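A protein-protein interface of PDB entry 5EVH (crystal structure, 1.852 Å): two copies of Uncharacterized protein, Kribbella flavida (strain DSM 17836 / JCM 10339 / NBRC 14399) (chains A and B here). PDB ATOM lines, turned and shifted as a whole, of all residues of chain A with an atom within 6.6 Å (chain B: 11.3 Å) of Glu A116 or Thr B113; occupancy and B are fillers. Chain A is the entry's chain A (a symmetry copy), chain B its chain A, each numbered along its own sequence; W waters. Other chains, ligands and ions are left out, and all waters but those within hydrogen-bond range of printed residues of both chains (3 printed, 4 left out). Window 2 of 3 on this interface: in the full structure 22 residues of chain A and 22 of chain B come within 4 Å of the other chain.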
ATOM      1  N   VAL A  87      -9.471  33.326  21.002  1.00  0.00           N
ATOM      2  CA  VAL A  87      -8.076  32.956  21.154  1.00  0.00           C
ATOM      3  C   VAL A  87      -7.232  34.054  20.518  1.00  0.00           C
ATOM      4  O   VAL A  87      -7.224  34.167  19.288  1.00  0.00           O
ATOM      5  CB  VAL A  87      -7.812  31.583  20.501  1.00  0.00           C
ATOM      6  CG1 VAL A  87      -6.322  31.214  20.633  1.00  0.00           C
ATOM      7  CG2 VAL A  87      -8.815  30.474  21.121  1.00  0.00           C
ATOM      8  N   ASP A 111      -3.207  24.159  16.867  1.00  0.00           N
ATOM      9  CA  ASP A 111      -3.525  23.577  18.172  1.00  0.00           C
ATOM     10  C   ASP A 111      -4.993  23.903  18.445  1.00  0.00           C
ATOM     11  O   ASP A 111      -5.361  25.088  18.565  1.00  0.00           O
ATOM     12  CB  ASP A 111      -2.627  24.179  19.244  1.00  0.00           C
ATOM     13  CG  ASP A 111      -2.901  23.612  20.632  1.00  0.00           C
ATOM     14  OD1 ASP A 111      -3.586  22.539  20.739  1.00  0.00           O
ATOM     15  OD2 ASP A 111      -2.409  24.212  21.634  1.00  0.00           O
ATOM     16  N   ARG A 112      -5.841  22.875  18.487  1.00  0.00           N
ATOM     17  CA  ARG A 112      -7.263  23.069  18.825  1.00  0.00           C
ATOM     18  C   ARG A 112      -7.519  23.340  20.316  1.00  0.00           C
ATOM     19  O   ARG A 112      -8.609  23.835  20.669  1.00  0.00           O
ATOM     20  CB  ARG A 112      -8.091  21.843  18.368  1.00  0.00           C
ATOM     21  CG  ARG A 112      -8.110  21.656  16.798  1.00  0.00           C
ATOM     22  CD  ARG A 112      -8.962  20.405  16.387  1.00  0.00           C
ATOM     23  NE  ARG A 112      -8.225  19.194  16.761  1.00  0.00           N
ATOM     24  CZ  ARG A 112      -8.758  17.994  16.884  1.00  0.00           C
ATOM     25  NH1 ARG A 112     -10.068  17.827  16.682  1.00  0.00           N
ATOM     26  NH2 ARG A 112      -7.985  16.979  17.219  1.00  0.00           N
ATOM     27  N   THR A 113      -6.553  23.047  21.191  1.00  0.00           N
ATOM     28  CA  THR A 113      -6.832  23.099  22.625  1.00  0.00           C
ATOM     29  C   THR A 113      -7.368  24.451  23.068  1.00  0.00           C
ATOM     30  O   THR A 113      -8.396  24.480  23.776  1.00  0.00           O
ATOM     31  CB  THR A 113      -5.580  22.671  23.408  1.00  0.00           C
ATOM     32  OG1 THR A 113      -5.299  21.310  23.068  1.00  0.00           O
ATOM     33  CG2 THR A 113      -5.795  22.746  24.931  1.00  0.00           C
ATOM     34  N   PRO A 114      -6.765  25.580  22.690  1.00  0.00           N
ATOM     35  CA  PRO A 114      -7.242  26.863  23.208  1.00  0.00           C
ATOM     36  C   PRO A 114      -8.688  27.119  22.863  1.00  0.00           C
ATOM     37  O   PRO A 114      -9.421  27.723  23.668  1.00  0.00           O
ATOM     38  CB  PRO A 114      -6.305  27.893  22.514  1.00  0.00           C
ATOM     39  CG  PRO A 114      -5.059  27.135  22.277  1.00  0.00           C
ATOM     40  CD  PRO A 114      -5.561  25.752  21.861  1.00  0.00           C
ATOM     41  N   PHE A 115      -9.125  26.683  21.677  1.00  0.00           N
ATOM     42  CA  PHE A 115     -10.514  26.885  21.280  1.00  0.00           C
ATOM     43  C   PHE A 115     -11.441  26.049  22.151  1.00  0.00           C
ATOM     44  O   PHE A 115     -12.403  26.565  22.745  1.00  0.00           O
ATOM     45  CB  PHE A 115     -10.682  26.563  19.801  1.00  0.00           C
ATOM     46  CG  PHE A 115      -9.901  27.480  18.890  1.00  0.00           C
ATOM     47  CD1 PHE A 115     -10.472  28.708  18.450  1.00  0.00           C
ATOM     48  CD2 PHE A 115      -8.593  27.180  18.514  1.00  0.00           C
ATOM     49  CE1 PHE A 115      -9.776  29.571  17.605  1.00  0.00           C
ATOM     50  CE2 PHE A 115      -7.894  28.016  17.660  1.00  0.00           C
ATOM     51  CZ  PHE A 115      -8.464  29.249  17.214  1.00  0.00           C
ATOM     52  N   GLU A 116     -11.119  24.766  22.292  1.00  0.00           N
ATOM     53  CA  GLU A 116     -11.920  23.890  23.138  1.00  0.00           C
ATOM     54  C   GLU A 116     -11.986  24.410  24.577  1.00  0.00           C
ATOM     55  O   GLU A 116     -13.052  24.384  25.208  1.00  0.00           O
ATOM     56  CB  GLU A 116     -11.307  22.488  23.047  1.00  0.00           C
ATOM     57  CG  GLU A 116     -12.009  21.407  23.865  1.00  0.00           C
ATOM     58  CD  GLU A 116     -11.312  20.046  23.646  1.00  0.00           C
ATOM     59  OE1 GLU A 116     -10.533  19.951  22.641  1.00  0.00           O
ATOM     60  OE2 GLU A 116     -11.509  19.103  24.475  1.00  0.00           O
ATOM     61  N   GLN A 117     -10.867  24.917  25.111  1.00  0.00           N
ATOM     62  CA  GLN A 117     -10.863  25.473  26.467  1.00  0.00           C
ATOM     63  C   GLN A 117     -11.755  26.704  26.563  1.00  0.00           C
ATOM     64  O   GLN A 117     -12.557  26.845  27.500  1.00  0.00           O
ATOM     65  CB  GLN A 117      -9.442  25.845  26.892  1.00  0.00           C
ATOM     66  CG  GLN A 117      -8.665  24.627  27.299  1.00  0.00           C
ATOM     67  CD  GLN A 117      -7.192  24.869  27.457  1.00  0.00           C
ATOM     68  OE1 GLN A 117      -6.641  25.912  27.047  1.00  0.00           O
ATOM     69  NE2 GLN A 117      -6.513  23.869  28.019  1.00  0.00           N
ATOM     70  N   ALA A 118     -11.610  27.626  25.615  1.00  0.00           N
ATOM     71  CA  ALA A 118     -12.495  28.785  25.596  1.00  0.00           C
ATOM     72  C   ALA A 118     -13.962  28.356  25.490  1.00  0.00           C
ATOM     73  O   ALA A 118     -14.833  28.930  26.155  1.00  0.00           O
ATOM     74  CB  ALA A 118     -12.099  29.726  24.443  1.00  0.00           C
ATOM     75  N   ARG A 119     -14.251  27.340  24.663  1.00  0.00           N
ATOM     76  CA  ARG A 119     -15.637  26.978  24.366  1.00  0.00           C
ATOM     77  C   ARG A 119     -16.282  26.260  25.540  1.00  0.00           C
ATOM     78  O   ARG A 119     -17.447  26.522  25.875  1.00  0.00           O
ATOM     79  CB  ARG A 119     -15.679  26.117  23.106  1.00  0.00           C
ATOM     80  CG  ARG A 119     -16.996  25.425  22.804  1.00  0.00           C
ATOM     81  CD  ARG A 119     -17.066  25.047  21.301  1.00  0.00           C
ATOM     82  NE  ARG A 119     -15.924  24.225  20.854  1.00  0.00           N
ATOM     83  CZ  ARG A 119     -14.994  24.598  19.961  1.00  0.00           C
ATOM     84  NH1 ARG A 119     -14.008  23.764  19.648  1.00  0.00           N
ATOM     85  NH2 ARG A 119     -15.042  25.793  19.374  1.00  0.00           N
ATOM     86  N   THR A 120     -15.531  25.371  26.192  1.00  0.00           N
ATOM     87  CA  THR A 120     -16.006  24.745  27.420  1.00  0.00           C
ATOM     88  C   THR A 120     -16.150  25.765  28.553  1.00  0.00           C
ATOM     89  O   THR A 120     -17.131  25.717  29.310  1.00  0.00           O
ATOM     90  CB  THR A 120     -15.064  23.612  27.826  1.00  0.00           C
ATOM     91  OG1 THR A 120     -15.005  22.641  26.769  1.00  0.00           O
ATOM     92  CG2 THR A 120     -15.557  22.936  29.093  1.00  0.00           C
ATOM     93  N   ALA A 121     -15.192  26.695  28.695  1.00  0.00           N
ATOM     94  CA  ALA A 121     -15.278  27.679  29.780  1.00  0.00           C
ATOM     95  C   ALA A 121     -16.506  28.574  29.624  1.00  0.00           C
ATOM     96  O   ALA A 121     -17.248  28.798  30.595  1.00  0.00           O
ATOM     97  CB  ALA A 121     -14.011  28.534  29.852  1.00  0.00           C
ATOM     98  N   PRO B  40       3.130  25.287  21.898  1.00  0.00           N
ATOM     99  CA  PRO B  40       1.675  25.468  22.051  1.00  0.00           C
ATOM    100  C   PRO B  40       1.256  25.848  23.455  1.00  0.00           C
ATOM    101  O   PRO B  40       0.327  26.654  23.604  1.00  0.00           O
ATOM    102  CB  PRO B  40       1.110  24.113  21.612  1.00  0.00           C
ATOM    103  CG  PRO B  40       2.111  23.685  20.528  1.00  0.00           C
ATOM    104  CD  PRO B  40       3.450  24.036  21.180  1.00  0.00           C
ATOM    105  N   ALA B  41       1.943  25.366  24.482  1.00  0.00           N
ATOM    106  CA  ALA B  41       1.560  25.706  25.843  1.00  0.00           C
ATOM    107  C   ALA B  41       2.154  27.030  26.311  1.00  0.00           C
ATOM    108  O   ALA B  41       1.775  27.508  27.382  1.00  0.00           O
ATOM    109  CB  ALA B  41       1.964  24.576  26.800  1.00  0.00           C
ATOM    110  N   PHE B  57       9.675  15.199  25.308  1.00  0.00           N
ATOM    111  CA  PHE B  57       8.967  15.098  24.030  1.00  0.00           C
ATOM    112  C   PHE B  57       9.614  14.017  23.190  1.00  0.00           C
ATOM    113  O   PHE B  57       8.938  13.086  22.704  1.00  0.00           O
ATOM    114  CB  PHE B  57       8.998  16.481  23.362  1.00  0.00           C
ATOM    115  CG  PHE B  57       8.019  16.696  22.215  1.00  0.00           C
ATOM    116  CD1 PHE B  57       7.278  15.666  21.673  1.00  0.00           C
ATOM    117  CD2 PHE B  57       7.876  17.993  21.675  1.00  0.00           C
ATOM    118  CE1 PHE B  57       6.393  15.908  20.594  1.00  0.00           C
ATOM    119  CE2 PHE B  57       6.982  18.249  20.599  1.00  0.00           C
ATOM    120  CZ  PHE B  57       6.244  17.212  20.072  1.00  0.00           C
ATOM    121  N   THR B  84       3.402   8.254  18.266  1.00  0.00           N
ATOM    122  CA  THR B  84       3.521   8.066  19.720  1.00  0.00           C
ATOM    123  C   THR B  84       2.623   6.899  20.112  1.00  0.00           C
ATOM    124  O   THR B  84       1.804   6.435  19.304  1.00  0.00           O
ATOM    125  CB  THR B  84       3.103   9.357  20.511  1.00  0.00           C
ATOM    126  OG1 THR B  84       1.684   9.518  20.431  1.00  0.00           O
ATOM    127  CG2 THR B  84       3.777  10.631  19.911  1.00  0.00           C
ATOM    128  N   PRO B  86       0.098   6.920  22.605  1.00  0.00           N
ATOM    129  CA  PRO B  86      -1.319   7.304  22.714  1.00  0.00           C
ATOM    130  C   PRO B  86      -1.892   7.879  21.446  1.00  0.00           C
ATOM    131  O   PRO B  86      -3.097   7.713  21.195  1.00  0.00           O
ATOM    132  CB  PRO B  86      -1.320   8.343  23.847  1.00  0.00           C
ATOM    133  CG  PRO B  86       0.077   8.925  23.858  1.00  0.00           C
ATOM    134  CD  PRO B  86       0.989   7.784  23.429  1.00  0.00           C
ATOM    135  N   VAL B  87      -1.063   8.493  20.612  1.00  0.00           N
ATOM    136  CA  VAL B  87      -1.553   9.186  19.433  1.00  0.00           C
ATOM    137  C   VAL B  87      -0.774   8.666  18.231  1.00  0.00           C
ATOM    138  O   VAL B  87       0.414   8.980  18.106  1.00  0.00           O
ATOM    139  CB  VAL B  87      -1.391  10.711  19.603  1.00  0.00           C
ATOM    140  CG1 VAL B  87      -1.877  11.438  18.335  1.00  0.00           C
ATOM    141  CG2 VAL B  87      -2.130  11.199  20.957  1.00  0.00           C
ATOM    142  N   PRO B  88      -1.432   7.962  17.304  1.00  0.00           N
ATOM    143  CA  PRO B  88      -0.711   7.316  16.179  1.00  0.00           C
ATOM    144  C   PRO B  88       0.049   8.289  15.318  1.00  0.00           C
ATOM    145  O   PRO B  88       1.159   7.963  14.859  1.00  0.00           O
ATOM    146  CB  PRO B  88      -1.840   6.662  15.362  1.00  0.00           C
ATOM    147  CG  PRO B  88      -2.999   6.563  16.289  1.00  0.00           C
ATOM    148  CD  PRO B  88      -2.880   7.681  17.294  1.00  0.00           C
ATOM    149  N   HIS B  89      -0.524   9.479  15.074  1.00  0.00           N
ATOM    150  CA  HIS B  89       0.093  10.515  14.222  1.00  0.00           C
ATOM    151  C   HIS B  89      -0.092  11.859  14.884  1.00  0.00           C
ATOM    152  O   HIS B  89      -1.228  12.290  15.094  1.00  0.00           O
ATOM    153  CB  HIS B  89      -0.538  10.558  12.833  1.00  0.00           C
ATOM    154  CG  HIS B  89      -0.196   9.353  12.019  1.00  0.00           C
ATOM    155  ND1 HIS B  89       1.047   9.210  11.411  1.00  0.00           N
ATOM    156  CD2 HIS B  89      -0.869   8.197  11.811  1.00  0.00           C
ATOM    157  CE1 HIS B  89       1.082   8.037  10.789  1.00  0.00           C
ATOM    158  NE2 HIS B  89      -0.056   7.393  11.043  1.00  0.00           N
ATOM    159  N   ALA B  90       1.005  12.539  15.165  1.00  0.00           N
ATOM    160  CA  ALA B  90       0.972  13.849  15.809  1.00  0.00           C
ATOM    161  C   ALA B  90       1.967  14.718  15.026  1.00  0.00           C
ATOM    162  O   ALA B  90       3.132  14.838  15.388  1.00  0.00           O
ATOM    163  CB  ALA B  90       1.355  13.702  17.280  1.00  0.00           C
ATOM    164  N   PRO B  91       1.556  15.272  13.896  1.00  0.00           N
ATOM    165  CA  PRO B  91       2.502  16.064  13.087  1.00  0.00           C
ATOM    166  C   PRO B  91       2.815  17.410  13.741  1.00  0.00           C
ATOM    167  O   PRO B  91       2.013  17.955  14.501  1.00  0.00           O
ATOM    168  CB  PRO B  91       1.759  16.252  11.767  1.00  0.00           C
ATOM    169  CG  PRO B  91       0.324  16.393  12.227  1.00  0.00           C
ATOM    170  CD  PRO B  91       0.211  15.216  13.290  1.00  0.00           C
ATOM    171  N   ILE B 109       4.505  24.201  16.301  1.00  0.00           N
ATOM    172  CA  ILE B 109       3.033  24.096  16.311  1.00  0.00           C
ATOM    173  C   ILE B 109       2.685  22.619  16.239  1.00  0.00           C
ATOM    174  O   ILE B 109       3.155  21.924  15.340  1.00  0.00           O
ATOM    175  CB  ILE B 109       2.398  24.831  15.111  1.00  0.00           C
ATOM    176  CG1 ILE B 109       2.862  26.288  15.100  1.00  0.00           C
ATOM    177  CG2 ILE B 109       0.867  24.713  15.258  1.00  0.00           C
ATOM    178  CD1 ILE B 109       2.280  27.103  13.858  1.00  0.00           C
ATOM    179  N   PHE B 110       1.841  22.151  17.157  1.00  0.00           N
ATOM    180  CA  PHE B 110       1.207  20.856  17.010  1.00  0.00           C
ATOM    181  C   PHE B 110      -0.088  20.885  17.812  1.00  0.00           C
ATOM    182  O   PHE B 110      -0.318  21.778  18.649  1.00  0.00           O
ATOM    183  CB  PHE B 110       2.094  19.708  17.496  1.00  0.00           C
ATOM    184  CG  PHE B 110       2.558  19.859  18.912  1.00  0.00           C
ATOM    185  CD1 PHE B 110       3.787  20.471  19.180  1.00  0.00           C
ATOM    186  CD2 PHE B 110       1.780  19.399  19.961  1.00  0.00           C
ATOM    187  CE1 PHE B 110       4.236  20.607  20.544  1.00  0.00           C
ATOM    188  CE2 PHE B 110       2.193  19.527  21.315  1.00  0.00           C
ATOM    189  CZ  PHE B 110       3.407  20.148  21.603  1.00  0.00           C
ATOM    190  N   ASP B 111      -0.954  19.932  17.525  1.00  0.00           N
ATOM    191  CA  ASP B 111      -2.298  19.921  18.104  1.00  0.00           C
ATOM    192  C   ASP B 111      -2.209  19.104  19.393  1.00  0.00           C
ATOM    193  O   ASP B 111      -1.909  17.895  19.349  1.00  0.00           O
ATOM    194  CB  ASP B 111      -3.281  19.289  17.129  1.00  0.00           C
ATOM    195  CG  ASP B 111      -4.707  19.250  17.666  1.00  0.00           C
ATOM    196  OD1 ASP B 111      -5.008  19.972  18.676  1.00  0.00           O
ATOM    197  OD2 ASP B 111      -5.555  18.523  17.068  1.00  0.00           O
ATOM    198  N   ARG B 112      -2.408  19.759  20.537  1.00  0.00           N
ATOM    199  CA  ARG B 112      -2.426  19.051  21.831  1.00  0.00           C
ATOM    200  C   ARG B 112      -3.704  18.234  22.077  1.00  0.00           C
ATOM    201  O   ARG B 112      -3.704  17.350  22.959  1.00  0.00           O
ATOM    202  CB  ARG B 112      -2.218  20.057  22.990  1.00  0.00           C
ATOM    203  CG  ARG B 112      -0.794  20.744  22.969  1.00  0.00           C
ATOM    204  CD  ARG B 112      -0.633  21.749  24.162  1.00  0.00           C
ATOM    205  NE  ARG B 112      -1.468  22.925  23.899  1.00  0.00           N
ATOM    206  CZ  ARG B 112      -1.847  23.800  24.810  1.00  0.00           C
ATOM    207  NH1 ARG B 112      -1.484  23.629  26.084  1.00  0.00           N
ATOM    208  NH2 ARG B 112      -2.594  24.824  24.445  1.00  0.00           N
ATOM    209  N   THR B 113      -4.777  18.489  21.324  1.00  0.00           N
ATOM    210  CA  THR B 113      -6.062  17.879  21.663  1.00  0.00           C
ATOM    211  C   THR B 113      -5.988  16.362  21.742  1.00  0.00           C
ATOM    212  O   THR B 113      -6.469  15.795  22.744  1.00  0.00           O
ATOM    213  CB  THR B 113      -7.138  18.369  20.680  1.00  0.00           C
ATOM    214  OG1 THR B 113      -7.269  19.784  20.850  1.00  0.00           O
ATOM    215  CG2 THR B 113      -8.511  17.728  20.955  1.00  0.00           C
ATOM    216  N   PRO B 114      -5.402  15.657  20.773  1.00  0.00           N
ATOM    217  CA  PRO B 114      -5.427  14.195  20.825  1.00  0.00           C
ATOM    218  C   PRO B 114      -4.781  13.654  22.076  1.00  0.00           C
ATOM    219  O   PRO B 114      -5.235  12.627  22.614  1.00  0.00           O
ATOM    220  CB  PRO B 114      -4.630  13.783  19.554  1.00  0.00           C
ATOM    221  CG  PRO B 114      -4.844  14.909  18.621  1.00  0.00           C
ATOM    222  CD  PRO B 114      -4.776  16.137  19.529  1.00  0.00           C
ATOM    223  N   PHE B 115      -3.721  14.312  22.556  1.00  0.00           N
ATOM    224  CA  PHE B 115      -3.051  13.854  23.767  1.00  0.00           C
ATOM    225  C   PHE B 115      -3.960  14.036  24.975  1.00  0.00           C
ATOM    226  O   PHE B 115      -4.202  13.090  25.745  1.00  0.00           O
ATOM    227  CB  PHE B 115      -1.728  14.588  23.937  1.00  0.00           C
ATOM    228  CG  PHE B 115      -0.733  14.303  22.836  1.00  0.00           C
ATOM    229  CD1 PHE B 115       0.140  13.183  22.933  1.00  0.00           C
ATOM    230  CD2 PHE B 115      -0.692  15.084  21.683  1.00  0.00           C
ATOM    231  CE1 PHE B 115       1.071  12.900  21.935  1.00  0.00           C
ATOM    232  CE2 PHE B 115       0.240  14.830  20.690  1.00  0.00           C
ATOM    233  CZ  PHE B 115       1.120  13.707  20.784  1.00  0.00           C
ATOM    234  N   GLU B 116      -4.526  15.231  25.112  1.00  0.00           N
ATOM    235  CA  GLU B 116      -5.444  15.495  26.213  1.00  0.00           C
ATOM    236  C   GLU B 116      -6.632  14.528  26.194  1.00  0.00           C
ATOM    237  O   GLU B 116      -7.050  14.024  27.246  1.00  0.00           O
ATOM    238  CB  GLU B 116      -5.877  16.960  26.101  1.00  0.00           C
ATOM    239  CG  GLU B 116      -6.847  17.446  27.175  1.00  0.00           C
ATOM    240  CD  GLU B 116      -7.162  18.943  26.962  1.00  0.00           C
ATOM    241  OE1 GLU B 116      -6.378  19.596  26.196  1.00  0.00           O
ATOM    242  OE2 GLU B 116      -8.186  19.451  27.517  1.00  0.00           O
ATOM    243  N   GLN B 117      -7.174  14.227  25.007  1.00  0.00           N
ATOM    244  CA  GLN B 117      -8.285  13.276  24.906  1.00  0.00           C
ATOM    245  C   GLN B 117      -7.860  11.878  25.338  1.00  0.00           C
ATOM    246  O   GLN B 117      -8.562  11.202  26.105  1.00  0.00           O
ATOM    247  CB  GLN B 117      -8.817  13.221  23.473  1.00  0.00           C
ATOM    248  CG  GLN B 117      -9.692  14.404  23.177  1.00  0.00           C
ATOM    249  CD  GLN B 117     -10.019  14.570  21.721  1.00  0.00           C
ATOM    250  OE1 GLN B 117      -9.419  13.937  20.828  1.00  0.00           O
ATOM    251  NE2 GLN B 117     -10.959  15.477  21.454  1.00  0.00           N
ATOM    252  N   ALA B 118      -6.720  11.414  24.831  1.00  0.00           N
ATOM    253  CA  ALA B 118      -6.209  10.122  25.273  1.00  0.00           C
ATOM    254  C   ALA B 118      -5.987  10.108  26.789  1.00  0.00           C
ATOM    255  O   ALA B 118      -6.293   9.114  27.458  1.00  0.00           O
ATOM    256  CB  ALA B 118      -4.914   9.784  24.510  1.00  0.00           C
ATOM    257  N   ARG B 119      -5.460  11.208  27.347  1.00  0.00           N
ATOM    258  CA  ARG B 119      -5.052  11.221  28.752  1.00  0.00           C
ATOM    259  C   ARG B 119      -6.258  11.280  29.675  1.00  0.00           C
ATOM    260  O   ARG B 119      -6.297  10.589  30.704  1.00  0.00           O
ATOM    261  CB  ARG B 119      -4.115  12.401  28.998  1.00  0.00           C
ATOM    262  CG  ARG B 119      -3.811  12.732  30.448  1.00  0.00           C
ATOM    263  CD  ARG B 119      -2.499  13.554  30.543  1.00  0.00           C
ATOM    264  NE  ARG B 119      -2.516  14.775  29.716  1.00  0.00           N
ATOM    265  CZ  ARG B 119      -1.725  15.017  28.659  1.00  0.00           C
ATOM    266  NH1 ARG B 119      -1.845  16.159  27.992  1.00  0.00           N
ATOM    267  NH2 ARG B 119      -0.811  14.130  28.265  1.00  0.00           N
ATOM    268  N   THR B 120      -7.262  12.079  29.309  1.00  0.00           N
ATOM    269  CA  THR B 120      -8.520  12.086  30.046  1.00  0.00           C
ATOM    270  C   THR B 120      -9.259  10.752  29.912  1.00  0.00           C
ATOM    271  O   THR B 120      -9.817  10.251  30.900  1.00  0.00           O
ATOM    272  CB  THR B 120      -9.397  13.243  29.566  1.00  0.00           C
ATOM    273  OG1 THR B 120      -8.700  14.483  29.767  1.00  0.00           O
ATOM    274  CG2 THR B 120     -10.704  13.278  30.338  1.00  0.00           C
ATOM    275  N   ALA B 121      -9.281  10.156  28.710  1.00  0.00           N
ATOM    276  CA  ALA B 121      -9.995   8.887  28.531  1.00  0.00           C
ATOM    277  C   ALA B 121      -9.375   7.776  29.376  1.00  0.00           C
ATOM    278  O   ALA B 121     -10.094   7.030  30.061  1.00  0.00           O
ATOM    279  CB  ALA B 121     -10.025   8.473  27.059  1.00  0.00           C
ATOM    280  N   ARG B 122      -8.037   7.645  29.340  1.00  0.00           N
ATOM    281  CA  ARG B 122      -7.357   6.653  30.182  1.00  0.00           C
ATOM    282  C   ARG B 122      -7.697   6.849  31.665  1.00  0.00           C
ATOM    283  O   ARG B 122      -8.034   5.884  32.366  1.00  0.00           O
ATOM    284  CB  ARG B 122      -5.838   6.708  29.960  1.00  0.00           C
ATOM    285  N   GLU B 124     -10.156   8.484  33.353  1.00  0.00           N
ATOM    286  CA  GLU B 124     -11.540   8.271  33.769  1.00  0.00           C
ATOM    287  C   GLU B 124     -12.094   6.907  33.353  1.00  0.00           C
ATOM    288  O   GLU B 124     -13.237   6.586  33.697  1.00  0.00           O
ATOM    289  CB  GLU B 124     -12.441   9.376  33.206  1.00  0.00           C
ATOM    290  CG  GLU B 124     -12.107  10.776  33.680  1.00  0.00           C
ATOM    291  CD  GLU B 124     -12.889  11.832  32.922  1.00  0.00           C
ATOM    292  OE1 GLU B 124     -13.658  11.459  32.014  1.00  0.00           O
ATOM    293  OE2 GLU B 124     -12.734  13.032  33.226  1.00  0.00           O
HETATM  294  O   HOH W   1      -1.263  26.842  21.264  1.00  0.00           O
HETATM  295  O   HOH W   2      -8.903  14.409  17.963  1.00  0.00           O
HETATM  296  O   HOH W   3      -3.897  26.603  26.217  1.00  0.00           O
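NE of Arg B112 lies within salt-bridge range of OD2 of Asp A111, 2.8 Å away. The side-chain hydroxyl (OG1) of Thr B113 is in hydrogen-bond range of the side-chain hydroxyl (OG1) of Thr A113, 3.3 Å away. The side-chain carboxylate (OD2) of Asp B111 is in salt-bridge range of the guanidinium group (NE) of Arg A112 (2.8 Å).
Water W3 bridges NH2 of Arg B112 (2.8 Å) and OE1 of Gln A117 (2.9 Å). Water W2 bridges the guanidinium group (NH2) of Arg A112 and the side-chain amide oxygen (OE1) of Gln B117. Water W1 bridges the backbone carbonyl oxygen of Pro B40 and the side-chain carboxylate of Asp A111.
Asp A111 touches its own counterpart, Asp B111. Asp A111 touches Arg B112, and with the chains exchanged Arg A112 touches Asp B111. Thr A113 touches its own counterpart, Thr B113. Thr A113 touches Glu B116, and with the chains exchanged Glu A116 touches Thr B113. Positions printed for both chains: 87, 111, 112, 113, 114, 115, 116, 117, 118, 119, 120 and 121. Of the 10 pairs that touch across the chains among the printed residues, 8 have their exchanged pair printed and touching as well.
Of chain B, only Pro B40, Phe B110, Asp B111 and Arg B112 come within 4 Å of Asp A111. Printed residues of chain B within 4 Å of Glu A116: Thr B113. No residue of chain B comes within 4 Å of Gln A117. No residue of chain B comes within 4 Å of Ala A118. Printed residues of chain A within 4 Å of Pro B40: Asp A111 (3.5 Å). Printed residues of chain A within 4 Å of Phe B110: Asp A111. Printed residues of chain A within 4 Å of Asp B111: Asp A111 and Arg A112. Of the printed residues of chain A, Thr B113 touches Arg A112 (3.3 Å), Thr A113 (3.3 Å) and Glu A116 (3.4 Å). Phe B115 touches none of the printed residues of chain A. Of the printed residues of chain A, Glu B116 touches Thr A113 (3.4 Å). Gln B117 touches none of the printed residues of chain A.
Hydrophobic or aromatic side chains of chain B that line the printed part of chain A: Pro B40. Of the 12 printed residues of chain A, 4 touch a printed residue of chain B.
The side-chain carboxylate (OD1) of Asp B111 lies within hydrogen-bond range of the backbone NH (N) of Thr B113, 3.0 Å away. O of Glu A116 is in hydrogen-bond range of OG1 of Thr A120, at 3.0 Å. The side-chain carboxylate (OD1) of Asp A111 is in hydrogen-bond range of the backbone NH (N) of Thr A113, at 3.0 Å. The side-chain hydroxyl (OG1) of Thr B120 is in hydrogen-bond range of the backbone carbonyl oxygen (O) of Glu B116 (3.0 Å).
Pro B40 touches Asp A111. Phe B110 touches Asp A111 (O to CB, 3.4 Å). Asp A111 touches Asp B111 (OD1 to OD1, 3.6 Å). CB of Arg A112 touches OG1 of Thr B113 (3.3 Å). CB of Arg B112 touches OG1 of Thr A113, 3.3 Å away. Thr A113 touches Glu B116 (CG2 to OE1, 3.4 Å). Glu A116 touches Thr B113.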
